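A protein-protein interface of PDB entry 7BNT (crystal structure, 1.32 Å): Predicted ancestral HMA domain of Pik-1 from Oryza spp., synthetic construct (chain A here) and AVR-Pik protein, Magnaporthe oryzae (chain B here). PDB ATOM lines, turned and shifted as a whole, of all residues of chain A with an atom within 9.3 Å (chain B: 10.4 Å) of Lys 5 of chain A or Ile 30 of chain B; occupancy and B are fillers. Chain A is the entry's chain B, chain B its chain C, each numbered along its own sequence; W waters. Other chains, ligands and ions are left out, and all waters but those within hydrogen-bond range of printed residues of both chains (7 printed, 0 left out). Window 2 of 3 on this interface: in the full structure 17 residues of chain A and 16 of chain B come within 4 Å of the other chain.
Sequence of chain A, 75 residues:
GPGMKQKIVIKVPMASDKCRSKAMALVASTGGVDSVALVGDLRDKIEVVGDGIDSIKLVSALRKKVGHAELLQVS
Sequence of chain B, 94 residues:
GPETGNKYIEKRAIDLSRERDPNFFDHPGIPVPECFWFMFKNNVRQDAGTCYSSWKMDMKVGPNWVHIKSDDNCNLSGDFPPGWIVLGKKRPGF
Gly 3 of chain A touches none of the printed residues of chain B. Of chain B, only Ile 30 comes within 4 Å of Lys 5 of chain A. No residue of chain B comes within 4 Å of Gly 50 of chain A. Ile 53 of chain A touches none of the printed residues of chain B. Printed residues of chain B within 4 Å of Ser 75 of chain A: Trp 55. Printed residues of chain A within 4 Å of Phe 25 of chain B: Glu 47 (3.9 Å). No residue of chain A comes within 4 Å of Gly 29 of chain B. Of chain A, only Lys 5 (3.5 Å) and Val 49 (3.8 Å) come within 4 Å of Ile 30 of chain B. No residue of chain A comes within 4 Å of Pro 31 of chain B. Of the printed residues of chain A, Trp 55 of chain B touches Gly 1 (3.3 Å), Pro 2 (3.3 Å) and Ser 75 (3.2 Å). The nearest printed residue of chain A that does not touch Ile 30 of chain B is Lys 7 of chain A (4.9 Å).
The side-chain hydroxyl (OG) of Ser 35 of chain A sits at hydrogen-bond distance from a ring nitrogen (ND1) of His 27 of chain B, 2.7 Å away. OE1 of Glu 47 of chain A sits at hydrogen-bond distance from NE2 of His 27 of chain B, at 2.7 Å. NE1 of Trp 55 of chain B is in hydrogen-bond range of OXT of Ser 75 of chain A (3.2 Å).
Printed residues of chain A that touch a printed residue of chain B: Gly 1, Pro 2, Lys 5, Ser 35, Glu 47, Val 49 and Ser 75. Hydrophobic or aromatic side chains of chain A within 4 Å of the printed part of chain B: Pro 2 and Val 49. Printed residues of chain B that touch a printed residue of chain A: Phe 25, His 27, Ile 30, Tyr 52 and Trp 55. Among the printed residues, 10 pairs touch across the chains.
Water W5 lies within hydrogen-bond range of OE1 of Glu 47 of chain A (2.7 Å), N of Phe 25 of chain B (2.9 Å) and OG1 of Thr 50 of chain B (3.4 Å). Water W3 lies within hydrogen-bond range of the side-chain carboxylate of Glu 47 of chain A (2.7 Å), the side-chain hydroxyl of Thr 50 of chain B (2.8 Å) and the side-chain amino group of Lys 7 of chain A (2.9 Å). Water W6 lies within hydrogen-bond range of O of Thr 50 of chain B (2.8 Å) and NZ of Lys 7 of chain A (2.9 Å). Water W2 bridges OH of Tyr 52 of chain B (3.0 Å) and O of Pro 2 of chain A (3.1 Å).
The chain-end carboxylate (OXT) of Ser 75 of chain A is in hydrogen-bond range of the backbone NH (N) of Gly 1 of chain A (2.8 Å). The side-chain carboxylate of Asp 34 of chain A is in salt-bridge range of the side-chain amino group of Lys 5 of chain A (2.7 Å). The side-chain carboxylate (OD2) of Asp 51 of chain A lies within salt-bridge range of the side-chain amino group (NZ) of Lys 5 of chain A (2.7 Å). O of Lys 7 of chain A sits at hydrogen-bond distance from N of Ser 75 of chain A. The side-chain hydroxyl (OH) of Tyr 52 of chain B is in hydrogen-bond range of the backbone carbonyl oxygen (O) of Pro 31 of chain B.
C of Gly 1 of chain A touches CZ2 of Trp 55 of chain B, at 3.3 Å. Tyr 52 of chain B touches Pro 2 of chain A (CD2 to CD, 3.6 Å). CZ2 of Trp 55 of chain B touches N of Pro 2 of chain A, 3.3 Å away. CB of Lys 5 of chain A touches CG2 of Ile 30 of chain B (3.5 Å). Glu 47 of chain A touches Phe 25 of chain B (OE1 to O, 3.9 Å). Val 49 of chain A touches His 27 of chain B. CG1 of Val 49 of chain A touches CG2 of Ile 30 of chain B, at 3.8 Å.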
ATOM      1  N   GLY A   1      14.878   2.406   0.990  1.00  0.00           N
ATOM      2  CA  GLY A   1      14.824   1.515  -0.209  1.00  0.00           C
ATOM      3  C   GLY A   1      13.560   0.724  -0.050  1.00  0.00           C
ATOM      4  O   GLY A   1      12.875   0.963   0.958  1.00  0.00           O
ATOM      5  N   PRO A   2      13.219  -0.200  -0.980  1.00  0.00           N
ATOM      6  CA  PRO A   2      11.989  -0.947  -0.812  1.00  0.00           C
ATOM      7  C   PRO A   2      12.028  -1.662   0.543  1.00  0.00           C
ATOM      8  O   PRO A   2      13.020  -2.252   0.893  1.00  0.00           O
ATOM      9  CB  PRO A   2      11.954  -1.922  -1.983  1.00  0.00           C
ATOM     10  CG  PRO A   2      13.053  -1.543  -2.913  1.00  0.00           C
ATOM     11  CD  PRO A   2      13.962  -0.614  -2.174  1.00  0.00           C
ATOM     12  N   GLY A   3      10.916  -1.605   1.256  1.00  0.00           N
ATOM     13  CA  GLY A   3      10.818  -2.175   2.602  1.00  0.00           C
ATOM     14  C   GLY A   3      10.960  -1.093   3.648  1.00  0.00           C
ATOM     15  O   GLY A   3      10.612   0.053   3.359  1.00  0.00           O
ATOM     16  N   MET A   4      11.387  -1.451   4.844  1.00  0.00           N
ATOM     17  CA  MET A   4      11.357  -0.513   5.989  1.00  0.00           C
ATOM     18  C   MET A   4      12.737   0.088   6.260  1.00  0.00           C
ATOM     19  O   MET A   4      12.825   0.953   7.121  1.00  0.00           O
ATOM     20  CB  MET A   4      10.761  -1.204   7.225  1.00  0.00           C
ATOM     21  CG  MET A   4       9.233  -1.264   7.160  1.00  0.00           C
ATOM     22  SD  MET A   4       8.438   0.402   7.003  1.00  0.00           S
ATOM     23  CE  MET A   4       9.014   1.155   8.520  1.00  0.00           C
ATOM     24  N   LYS A   5      13.750  -0.226   5.472  1.00  0.00           N
ATOM     25  CA  LYS A   5      15.100   0.320   5.743  1.00  0.00           C
ATOM     26  C   LYS A   5      15.358   1.525   4.833  1.00  0.00           C
ATOM     27  O   LYS A   5      14.827   1.609   3.738  1.00  0.00           O
ATOM     28  CB  LYS A   5      16.168  -0.748   5.528  1.00  0.00           C
ATOM     29  CG  LYS A   5      15.987  -2.015   6.361  1.00  0.00           C
ATOM     30  CD  LYS A   5      16.182  -1.785   7.825  1.00  0.00           C
ATOM     31  CE  LYS A   5      16.078  -3.082   8.613  1.00  0.00           C
ATOM     32  NZ  LYS A   5      16.419  -2.887  10.032  1.00  0.00           N
ATOM     33  N   GLN A   6      16.147   2.447   5.359  1.00  0.00           N
ATOM     34  CA  GLN A   6      16.674   3.624   4.663  1.00  0.00           C
ATOM     35  C   GLN A   6      18.077   3.301   4.145  1.00  0.00           C
ATOM     36  O   GLN A   6      18.788   2.514   4.752  1.00  0.00           O
ATOM     37  CB  GLN A   6      16.847   4.780   5.651  1.00  0.00           C
ATOM     38  CG  GLN A   6      15.586   5.246   6.363  1.00  0.00           C
ATOM     39  CD  GLN A   6      16.003   6.123   7.510  1.00  0.00           C
ATOM     40  OE1 GLN A   6      16.257   5.617   8.605  1.00  0.00           O
ATOM     41  NE2 GLN A   6      16.114   7.425   7.255  1.00  0.00           N
ATOM     42  N   LYS A   7      18.451   3.857   3.010  1.00  0.00           N
ATOM     43  CA  LYS A   7      19.858   3.855   2.569  1.00  0.00           C
ATOM     44  C   LYS A   7      20.213   5.302   2.275  1.00  0.00           C
ATOM     45  O   LYS A   7      19.490   5.970   1.536  1.00  0.00           O
ATOM     46  CB  LYS A   7      20.126   2.988   1.335  1.00  0.00           C
ATOM     47  CG  LYS A   7      21.584   3.006   0.881  1.00  0.00           C
ATOM     48  CD  LYS A   7      21.886   2.050  -0.265  1.00  0.00           C
ATOM     49  CE  LYS A   7      20.834   2.106  -1.343  1.00  0.00           C
ATOM     50  NZ  LYS A   7      21.191   1.288  -2.523  1.00  0.00           N
ATOM     51  N   ILE A   8      21.292   5.770   2.867  1.00  0.00           N
ATOM     52  CA  ILE A   8      21.824   7.096   2.498  1.00  0.00           C
ATOM     53  C   ILE A   8      23.321   6.959   2.254  1.00  0.00           C
ATOM     54  O   ILE A   8      23.975   5.997   2.701  1.00  0.00           O
ATOM     55  CB  ILE A   8      21.525   8.150   3.571  1.00  0.00           C
ATOM     56  CG1 ILE A   8      22.268   7.800   4.853  1.00  0.00           C
ATOM     57  CG2 ILE A   8      20.024   8.343   3.794  1.00  0.00           C
ATOM     58  CD1 ILE A   8      22.145   8.841   5.909  1.00  0.00           C
ATOM     59  N   GLY A  32      20.230   2.655  15.317  1.00  0.00           N
ATOM     60  CA  GLY A  32      19.396   2.206  14.185  1.00  0.00           C
ATOM     61  C   GLY A  32      20.184   1.905  12.930  1.00  0.00           C
ATOM     62  O   GLY A  32      19.567   1.656  11.926  1.00  0.00           O
ATOM     63  N   VAL A  33      21.501   1.987  12.974  1.00  0.00           N
ATOM     64  CA  VAL A  33      22.365   1.578  11.839  1.00  0.00           C
ATOM     65  C   VAL A  33      22.516   0.064  11.837  1.00  0.00           C
ATOM     66  O   VAL A  33      22.873  -0.521  12.859  1.00  0.00           O
ATOM     67  CB  VAL A  33      23.717   2.304  11.879  1.00  0.00           C
ATOM     68  CG1 VAL A  33      24.702   1.722  10.865  1.00  0.00           C
ATOM     69  CG2 VAL A  33      23.491   3.796  11.678  1.00  0.00           C
ATOM     70  N   ASP A  34      22.276  -0.546  10.695  1.00  0.00           N
ATOM     71  CA  ASP A  34      22.485  -1.988  10.465  1.00  0.00           C
ATOM     72  C   ASP A  34      23.829  -2.232   9.791  1.00  0.00           C
ATOM     73  O   ASP A  34      24.459  -3.247  10.127  1.00  0.00           O
ATOM     74  CB  ASP A  34      21.363  -2.561   9.632  1.00  0.00           C
ATOM     75  CG  ASP A  34      20.024  -2.455  10.331  1.00  0.00           C
ATOM     76  OD1 ASP A  34      20.009  -2.462  11.582  1.00  0.00           O
ATOM     77  OD2 ASP A  34      19.063  -2.294   9.606  1.00  0.00           O
ATOM     78  N   SER A  35      24.230  -1.394   8.854  1.00  0.00           N
ATOM     79  CA  SER A  35      25.452  -1.679   8.090  1.00  0.00           C
ATOM     80  C   SER A  35      26.002  -0.388   7.505  1.00  0.00           C
ATOM     81  O   SER A  35      25.237   0.543   7.212  1.00  0.00           O
ATOM     82  CB  SER A  35      25.242  -2.749   7.033  1.00  0.00           C
ATOM     83  OG  SER A  35      24.137  -2.425   6.215  1.00  0.00           O
ATOM     84  N   GLU A  47      28.143   4.588   2.737  1.00  0.00           N
ATOM     85  CA  GLU A  47      26.751   4.156   2.517  1.00  0.00           C
ATOM     86  C   GLU A  47      26.259   3.489   3.792  1.00  0.00           C
ATOM     87  O   GLU A  47      26.895   2.536   4.265  1.00  0.00           O
ATOM     88  CB  GLU A  47      26.727   3.193   1.358  1.00  0.00           C
ATOM     89  CG  GLU A  47      25.371   2.840   0.852  1.00  0.00           C
ATOM     90  CD  GLU A  47      25.579   2.020  -0.427  1.00  0.00           C
ATOM     91  OE1 GLU A  47      25.765   0.797  -0.338  1.00  0.00           O
ATOM     92  OE2 GLU A  47      25.661   2.621  -1.531  1.00  0.00           O
ATOM     93  N   VAL A  48      25.172   3.994   4.349  1.00  0.00           N
ATOM     94  CA  VAL A  48      24.655   3.443   5.625  1.00  0.00           C
ATOM     95  C   VAL A  48      23.201   3.047   5.409  1.00  0.00           C
ATOM     96  O   VAL A  48      22.445   3.778   4.745  1.00  0.00           O
ATOM     97  CB  VAL A  48      24.837   4.408   6.805  1.00  0.00           C
ATOM     98  CG1 VAL A  48      24.178   5.738   6.533  1.00  0.00           C
ATOM     99  CG2 VAL A  48      24.320   3.805   8.099  1.00  0.00           C
ATOM    100  N   VAL A  49      22.876   1.885   5.968  1.00  0.00           N
ATOM    101  CA  VAL A  49      21.543   1.254   5.888  1.00  0.00           C
ATOM    102  C   VAL A  49      21.052   1.035   7.315  1.00  0.00           C
ATOM    103  O   VAL A  49      21.807   0.571   8.186  1.00  0.00           O
ATOM    104  CB  VAL A  49      21.583  -0.044   5.080  1.00  0.00           C
ATOM    105  CG1 VAL A  49      20.307  -0.854   5.201  1.00  0.00           C
ATOM    106  CG2 VAL A  49      21.879   0.273   3.639  1.00  0.00           C
ATOM    107  N   GLY A  50      19.803   1.362   7.536  1.00  0.00           N
ATOM    108  CA  GLY A  50      19.194   1.104   8.829  1.00  0.00           C
ATOM    109  C   GLY A  50      17.817   1.693   8.891  1.00  0.00           C
ATOM    110  O   GLY A  50      17.214   1.909   7.885  1.00  0.00           O
ATOM    111  N   ASP A  51      17.321   1.880  10.079  1.00  0.00           N
ATOM    112  CA  ASP A  51      15.984   2.486  10.200  1.00  0.00           C
ATOM    113  C   ASP A  51      16.026   3.531  11.305  1.00  0.00           C
ATOM    114  O   ASP A  51      16.831   3.434  12.229  1.00  0.00           O
ATOM    115  CB  ASP A  51      14.941   1.383  10.307  1.00  0.00           C
ATOM    116  CG  ASP A  51      15.198   0.481  11.475  1.00  0.00           C
ATOM    117  OD1 ASP A  51      15.159   1.005  12.592  1.00  0.00           O
ATOM    118  OD2 ASP A  51      15.448  -0.728  11.262  1.00  0.00           O
ATOM    119  N   GLY A  52      15.224   4.567  11.128  1.00  0.00           N
ATOM    120  CA  GLY A  52      15.132   5.678  12.089  1.00  0.00           C
ATOM    121  C   GLY A  52      16.414   6.495  12.117  1.00  0.00           C
ATOM    122  O   GLY A  52      16.710   7.108  13.150  1.00  0.00           O
ATOM    123  N   ILE A  53      17.191   6.489  11.036  1.00  0.00           N
ATOM    124  CA  ILE A  53      18.426   7.320  10.958  1.00  0.00           C
ATOM    125  C   ILE A  53      18.028   8.709  10.521  1.00  0.00           C
ATOM    126  O   ILE A  53      17.289   8.861   9.550  1.00  0.00           O
ATOM    127  CB  ILE A  53      19.479   6.734  10.026  1.00  0.00           C
ATOM    128  CG1 ILE A  53      19.908   5.347  10.486  1.00  0.00           C
ATOM    129  CG2 ILE A  53      20.671   7.682   9.897  1.00  0.00           C
ATOM    130  CD1 ILE A  53      20.386   4.522   9.348  1.00  0.00           C
ATOM    131  N   VAL A  74      19.768   9.695  -1.003  1.00  0.00           N
ATOM    132  CA  VAL A  74      18.732   9.100  -0.129  1.00  0.00           C
ATOM    133  C   VAL A  74      17.908   8.176  -1.012  1.00  0.00           C
ATOM    134  O   VAL A  74      17.400   8.613  -2.064  1.00  0.00           O
ATOM    135  CB  VAL A  74      17.866  10.202   0.504  1.00  0.00           C
ATOM    136  CG1 VAL A  74      16.778   9.614   1.373  1.00  0.00           C
ATOM    137  CG2 VAL A  74      18.713  11.190   1.292  1.00  0.00           C
ATOM    138  N   SER A  75      17.759   6.933  -0.594  1.00  0.00           N
ATOM    139  CA  SER A  75      16.970   5.968  -1.377  1.00  0.00           C
ATOM    140  C   SER A  75      16.302   4.948  -0.464  1.00  0.00           C
ATOM    141  O   SER A  75      16.591   4.873   0.717  1.00  0.00           O
ATOM    142  CB  SER A  75      17.823   5.352  -2.406  1.00  0.00           C
ATOM    143  OG  SER A  75      18.897   4.657  -1.839  1.00  0.00           O
ATOM    144  OXT SER A  75      15.409   4.245  -1.001  1.00  0.00           O
ATOM    145  N   PHE B  25      28.615  -2.610  -1.918  1.00  0.00           N
ATOM    146  CA  PHE B  25      28.396  -3.568  -0.824  1.00  0.00           C
ATOM    147  C   PHE B  25      26.932  -3.929  -0.837  1.00  0.00           C
ATOM    148  O   PHE B  25      26.096  -3.045  -0.692  1.00  0.00           O
ATOM    149  CB  PHE B  25      28.778  -2.952   0.510  1.00  0.00           C
ATOM    150  CG  PHE B  25      28.512  -3.865   1.677  1.00  0.00           C
ATOM    151  CD1 PHE B  25      29.091  -5.129   1.761  1.00  0.00           C
ATOM    152  CD2 PHE B  25      27.666  -3.463   2.697  1.00  0.00           C
ATOM    153  CE1 PHE B  25      28.856  -5.946   2.853  1.00  0.00           C
ATOM    154  CE2 PHE B  25      27.450  -4.275   3.797  1.00  0.00           C
ATOM    155  CZ  PHE B  25      28.020  -5.516   3.859  1.00  0.00           C
ATOM    156  N   ASP B  26      26.647  -5.218  -0.988  1.00  0.00           N
ATOM    157  CA  ASP B  26      25.240  -5.658  -0.967  1.00  0.00           C
ATOM    158  C   ASP B  26      24.876  -5.878   0.497  1.00  0.00           C
ATOM    159  O   ASP B  26      25.033  -6.974   1.018  1.00  0.00           O
ATOM    160  CB  ASP B  26      25.038  -6.857  -1.877  1.00  0.00           C
ATOM    161  CG  ASP B  26      25.186  -6.496  -3.346  1.00  0.00           C
ATOM    162  OD1 ASP B  26      24.719  -5.381  -3.744  1.00  0.00           O
ATOM    163  OD2 ASP B  26      25.740  -7.329  -4.100  1.00  0.00           O
ATOM    164  N   HIS B  27      24.398  -4.831   1.147  1.00  0.00           N
ATOM    165  CA  HIS B  27      24.056  -4.860   2.583  1.00  0.00           C
ATOM    166  C   HIS B  27      23.126  -6.027   2.847  1.00  0.00           C
ATOM    167  O   HIS B  27      22.157  -6.213   2.128  1.00  0.00           O
ATOM    168  CB  HIS B  27      23.349  -3.572   2.985  1.00  0.00           C
ATOM    169  CG  HIS B  27      24.144  -2.339   2.722  1.00  0.00           C
ATOM    170  ND1 HIS B  27      24.806  -1.682   3.720  1.00  0.00           N
ATOM    171  CD2 HIS B  27      24.410  -1.665   1.573  1.00  0.00           C
ATOM    172  CE1 HIS B  27      25.432  -0.645   3.194  1.00  0.00           C
ATOM    173  NE2 HIS B  27      25.204  -0.608   1.887  1.00  0.00           N
ATOM    174  N   PRO B  28      23.366  -6.806   3.923  1.00  0.00           N
ATOM    175  CA  PRO B  28      22.574  -7.998   4.142  1.00  0.00           C
ATOM    176  C   PRO B  28      21.144  -7.710   4.591  1.00  0.00           C
ATOM    177  O   PRO B  28      20.302  -8.621   4.436  1.00  0.00           O
ATOM    178  CB  PRO B  28      23.336  -8.792   5.199  1.00  0.00           C
ATOM    179  CG  PRO B  28      24.330  -7.860   5.794  1.00  0.00           C
ATOM    180  CD  PRO B  28      24.533  -6.742   4.802  1.00  0.00           C
ATOM    181  N   GLY B  29      20.856  -6.538   5.147  1.00  0.00           N
ATOM    182  CA  GLY B  29      19.493  -6.320   5.711  1.00  0.00           C
ATOM    183  C   GLY B  29      18.409  -5.940   4.683  1.00  0.00           C
ATOM    184  O   GLY B  29      17.237  -5.732   5.062  1.00  0.00           O
ATOM    185  N   ILE B  30      18.765  -5.838   3.410  1.00  0.00           N
ATOM    186  CA  ILE B  30      17.894  -5.278   2.346  1.00  0.00           C
ATOM    187  C   ILE B  30      18.051  -6.103   1.075  1.00  0.00           C
ATOM    188  O   ILE B  30      19.055  -6.774   0.866  1.00  0.00           O
ATOM    189  CB  ILE B  30      18.210  -3.801   2.110  1.00  0.00           C
ATOM    190  CG1 ILE B  30      19.689  -3.574   1.764  1.00  0.00           C
ATOM    191  CG2 ILE B  30      17.800  -2.996   3.329  1.00  0.00           C
ATOM    192  CD1 ILE B  30      19.989  -2.160   1.356  1.00  0.00           C
ATOM    193  N   PRO B  31      17.049  -6.060   0.178  1.00  0.00           N
ATOM    194  CA  PRO B  31      17.183  -6.760  -1.090  1.00  0.00           C
ATOM    195  C   PRO B  31      18.399  -6.277  -1.888  1.00  0.00           C
ATOM    196  O   PRO B  31      18.868  -5.145  -1.738  1.00  0.00           O
ATOM    197  CB  PRO B  31      15.891  -6.489  -1.855  1.00  0.00           C
ATOM    198  CG  PRO B  31      14.996  -5.769  -0.909  1.00  0.00           C
ATOM    199  CD  PRO B  31      15.745  -5.413   0.346  1.00  0.00           C
ATOM    200  N   VAL B  32      18.918  -7.170  -2.704  1.00  0.00           N
ATOM    201  CA  VAL B  32      20.121  -6.848  -3.512  1.00  0.00           C
ATOM    202  C   VAL B  32      19.680  -5.979  -4.673  1.00  0.00           C
ATOM    203  O   VAL B  32      18.828  -6.360  -5.487  1.00  0.00           O
ATOM    204  CB  VAL B  32      20.824  -8.114  -4.009  1.00  0.00           C
ATOM    205  CG1 VAL B  32      21.977  -7.747  -4.934  1.00  0.00           C
ATOM    206  CG2 VAL B  32      21.284  -8.977  -2.846  1.00  0.00           C
ATOM    207  N   PRO B  33      20.241  -4.767  -4.811  1.00  0.00           N
ATOM    208  CA  PRO B  33      19.857  -3.920  -5.934  1.00  0.00           C
ATOM    209  C   PRO B  33      20.289  -4.482  -7.291  1.00  0.00           C
ATOM    210  O   PRO B  33      21.326  -5.126  -7.394  1.00  0.00           O
ATOM    211  CB  PRO B  33      20.526  -2.573  -5.635  1.00  0.00           C
ATOM    212  CG  PRO B  33      21.661  -2.933  -4.723  1.00  0.00           C
ATOM    213  CD  PRO B  33      21.244  -4.161  -3.947  1.00  0.00           C
ATOM    214  N   GLU B  34      19.436  -4.284  -8.286  1.00  0.00           N
ATOM    215  CA  GLU B  34      19.536  -4.962  -9.599  1.00  0.00           C
ATOM    216  C   GLU B  34      20.429  -4.197 -10.590  1.00  0.00           C
ATOM    217  O   GLU B  34      20.782  -4.764 -11.638  1.00  0.00           O
ATOM    218  CB  GLU B  34      18.138  -5.096 -10.202  1.00  0.00           C
ATOM    219  CG  GLU B  34      17.157  -5.844  -9.316  1.00  0.00           C
ATOM    220  CD  GLU B  34      16.351  -5.031  -8.317  1.00  0.00           C
ATOM    221  OE1 GLU B  34      16.690  -3.862  -8.074  1.00  0.00           O
ATOM    222  OE2 GLU B  34      15.383  -5.578  -7.761  1.00  0.00           O
ATOM    223  N   THR B  50      25.393   1.192  -7.003  1.00  0.00           N
ATOM    224  CA  THR B  50      24.235   0.317  -7.270  1.00  0.00           C
ATOM    225  C   THR B  50      22.934   1.073  -7.004  1.00  0.00           C
ATOM    226  O   THR B  50      22.903   2.027  -6.206  1.00  0.00           O
ATOM    227  CB  THR B  50      24.294  -0.961  -6.437  1.00  0.00           C
ATOM    228  OG1 THR B  50      24.331  -0.622  -5.055  1.00  0.00           O
ATOM    229  CG2 THR B  50      25.481  -1.820  -6.795  1.00  0.00           C
ATOM    230  N   CYS B  51      21.855   0.597  -7.633  1.00  0.00           N
ATOM    231  CA  CYS B  51      20.513   1.109  -7.337  1.00  0.00           C
ATOM    232  C   CYS B  51      19.482   0.056  -7.704  1.00  0.00           C
ATOM    233  O   CYS B  51      19.768  -0.853  -8.459  1.00  0.00           O
ATOM    234  CB  CYS B  51      20.245   2.456  -8.003  1.00  0.00           C
ATOM    235  SG  CYS B  51      20.258   2.430  -9.809  1.00  0.00           S
ATOM    236  N   TYR B  52      18.306   0.226  -7.140  1.00  0.00           N
ATOM    237  CA  TYR B  52      17.180  -0.683  -7.432  1.00  0.00           C
ATOM    238  C   TYR B  52      16.573  -0.353  -8.784  1.00  0.00           C
ATOM    239  O   TYR B  52      16.417   0.808  -9.130  1.00  0.00           O
ATOM    240  CB  TYR B  52      16.128  -0.556  -6.338  1.00  0.00           C
ATOM    241  CG  TYR B  52      16.592  -1.161  -5.041  1.00  0.00           C
ATOM    242  CD1 TYR B  52      16.653  -2.539  -4.878  1.00  0.00           C
ATOM    243  CD2 TYR B  52      17.003  -0.364  -3.994  1.00  0.00           C
ATOM    244  CE1 TYR B  52      17.125  -3.109  -3.703  1.00  0.00           C
ATOM    245  CE2 TYR B  52      17.457  -0.923  -2.810  1.00  0.00           C
ATOM    246  CZ  TYR B  52      17.527  -2.290  -2.660  1.00  0.00           C
ATOM    247  OH  TYR B  52      17.955  -2.757  -1.449  1.00  0.00           O
ATOM    248  N   TRP B  55      12.296   1.763  -9.188  1.00  0.00           N
ATOM    249  CA  TRP B  55      12.402   2.454  -7.884  1.00  0.00           C
ATOM    250  C   TRP B  55      12.760   3.913  -8.139  1.00  0.00           C
ATOM    251  O   TRP B  55      12.610   4.427  -9.269  1.00  0.00           O
ATOM    252  CB  TRP B  55      13.380   1.686  -6.962  1.00  0.00           C
ATOM    253  CG  TRP B  55      13.382   2.074  -5.511  1.00  0.00           C
ATOM    254  CD1 TRP B  55      14.382   2.664  -4.781  1.00  0.00           C
ATOM    255  CD2 TRP B  55      12.285   1.920  -4.620  1.00  0.00           C
ATOM    256  NE1 TRP B  55      13.982   2.875  -3.490  1.00  0.00           N
ATOM    257  CE2 TRP B  55      12.677   2.485  -3.381  1.00  0.00           C
ATOM    258  CE3 TRP B  55      10.996   1.399  -4.766  1.00  0.00           C
ATOM    259  CZ2 TRP B  55      11.838   2.464  -2.268  1.00  0.00           C
ATOM    260  CZ3 TRP B  55      10.160   1.392  -3.652  1.00  0.00           C
ATOM    261  CH2 TRP B  55      10.579   1.923  -2.435  1.00  0.00           C
ATOM    262  N   LYS B  56      13.213   4.577  -7.103  1.00  0.00           N
ATOM    263  CA  LYS B  56      13.480   6.016  -7.166  1.00  0.00           C
ATOM    264  C   LYS B  56      14.489   6.353  -6.085  1.00  0.00           C
ATOM    265  O   LYS B  56      14.541   5.672  -5.049  1.00  0.00           O
ATOM    266  CB  LYS B  56      12.188   6.811  -7.025  1.00  0.00           C
ATOM    267  CG  LYS B  56      11.551   6.832  -5.647  1.00  0.00           C
ATOM    268  CD  LYS B  56      11.040   5.482  -5.193  1.00  0.00           C
ATOM    269  CE  LYS B  56       9.983   5.587  -4.111  1.00  0.00           C
ATOM    270  NZ  LYS B  56      10.526   6.085  -2.833  1.00  0.00           N
ATOM    271  N   ARG B  91      22.964  -5.261 -13.571  1.00  0.00           N
ATOM    272  CA  ARG B  91      24.092  -6.006 -12.991  1.00  0.00           C
ATOM    273  C   ARG B  91      24.141  -7.416 -13.552  1.00  0.00           C
ATOM    274  O   ARG B  91      23.121  -7.944 -13.983  1.00  0.00           O
ATOM    275  CB  ARG B  91      23.932  -6.081 -11.483  1.00  0.00           C
ATOM    276  CG  ARG B  91      24.153  -4.740 -10.811  1.00  0.00           C
ATOM    277  CD  ARG B  91      23.880  -4.824  -9.328  1.00  0.00           C
ATOM    278  NE  ARG B  91      24.940  -5.560  -8.657  1.00  0.00           N
ATOM    279  CZ  ARG B  91      25.026  -5.728  -7.352  1.00  0.00           C
ATOM    280  NH1 ARG B  91      24.051  -5.308  -6.562  1.00  0.00           N
ATOM    281  NH2 ARG B  91      26.090  -6.306  -6.833  1.00  0.00           N
ATOM    282  N   PHE B  94      21.196 -10.345 -13.304  1.00  0.00           N
ATOM    283  CA  PHE B  94      19.861  -9.706 -13.242  1.00  0.00           C
ATOM    284  C   PHE B  94      19.296  -9.599 -14.666  1.00  0.00           C
ATOM    285  O   PHE B  94      19.267  -8.554 -15.319  1.00  0.00           O
ATOM    286  CB  PHE B  94      19.977  -8.403 -12.450  1.00  0.00           C
ATOM    287  CG  PHE B  94      20.239  -8.597 -10.974  1.00  0.00           C
ATOM    288  CD1 PHE B  94      19.185  -8.736 -10.080  1.00  0.00           C
ATOM    289  CD2 PHE B  94      21.531  -8.627 -10.466  1.00  0.00           C
ATOM    290  CE1 PHE B  94      19.422  -8.888  -8.719  1.00  0.00           C
ATOM    291  CE2 PHE B  94      21.765  -8.757  -9.104  1.00  0.00           C
ATOM    292  CZ  PHE B  94      20.712  -8.900  -8.234  1.00  0.00           C
ATOM    293  OXT PHE B  94      18.852 -10.648 -15.172  1.00  0.00           O
HETATM  294  O   HOH W   1      13.455   5.966  -2.478  1.00  0.00           O
HETATM  295  O   HOH W   2      15.990  -1.666   0.466  1.00  0.00           O
HETATM  296  O   HOH W   3      23.975   1.556  -3.412  1.00  0.00           O
HETATM  297  O   HOH W   4      22.152  -4.326   6.485  1.00  0.00           O
HETATM  298  O   HOH W   5      26.609  -0.591  -2.524  1.00  0.00           O
HETATM  299  O   HOH W   6      20.983   3.297  -4.592  1.00  0.00           O
HETATM  300  O   HOH W   7      20.708  -1.346  -1.780  1.00  0.00           O
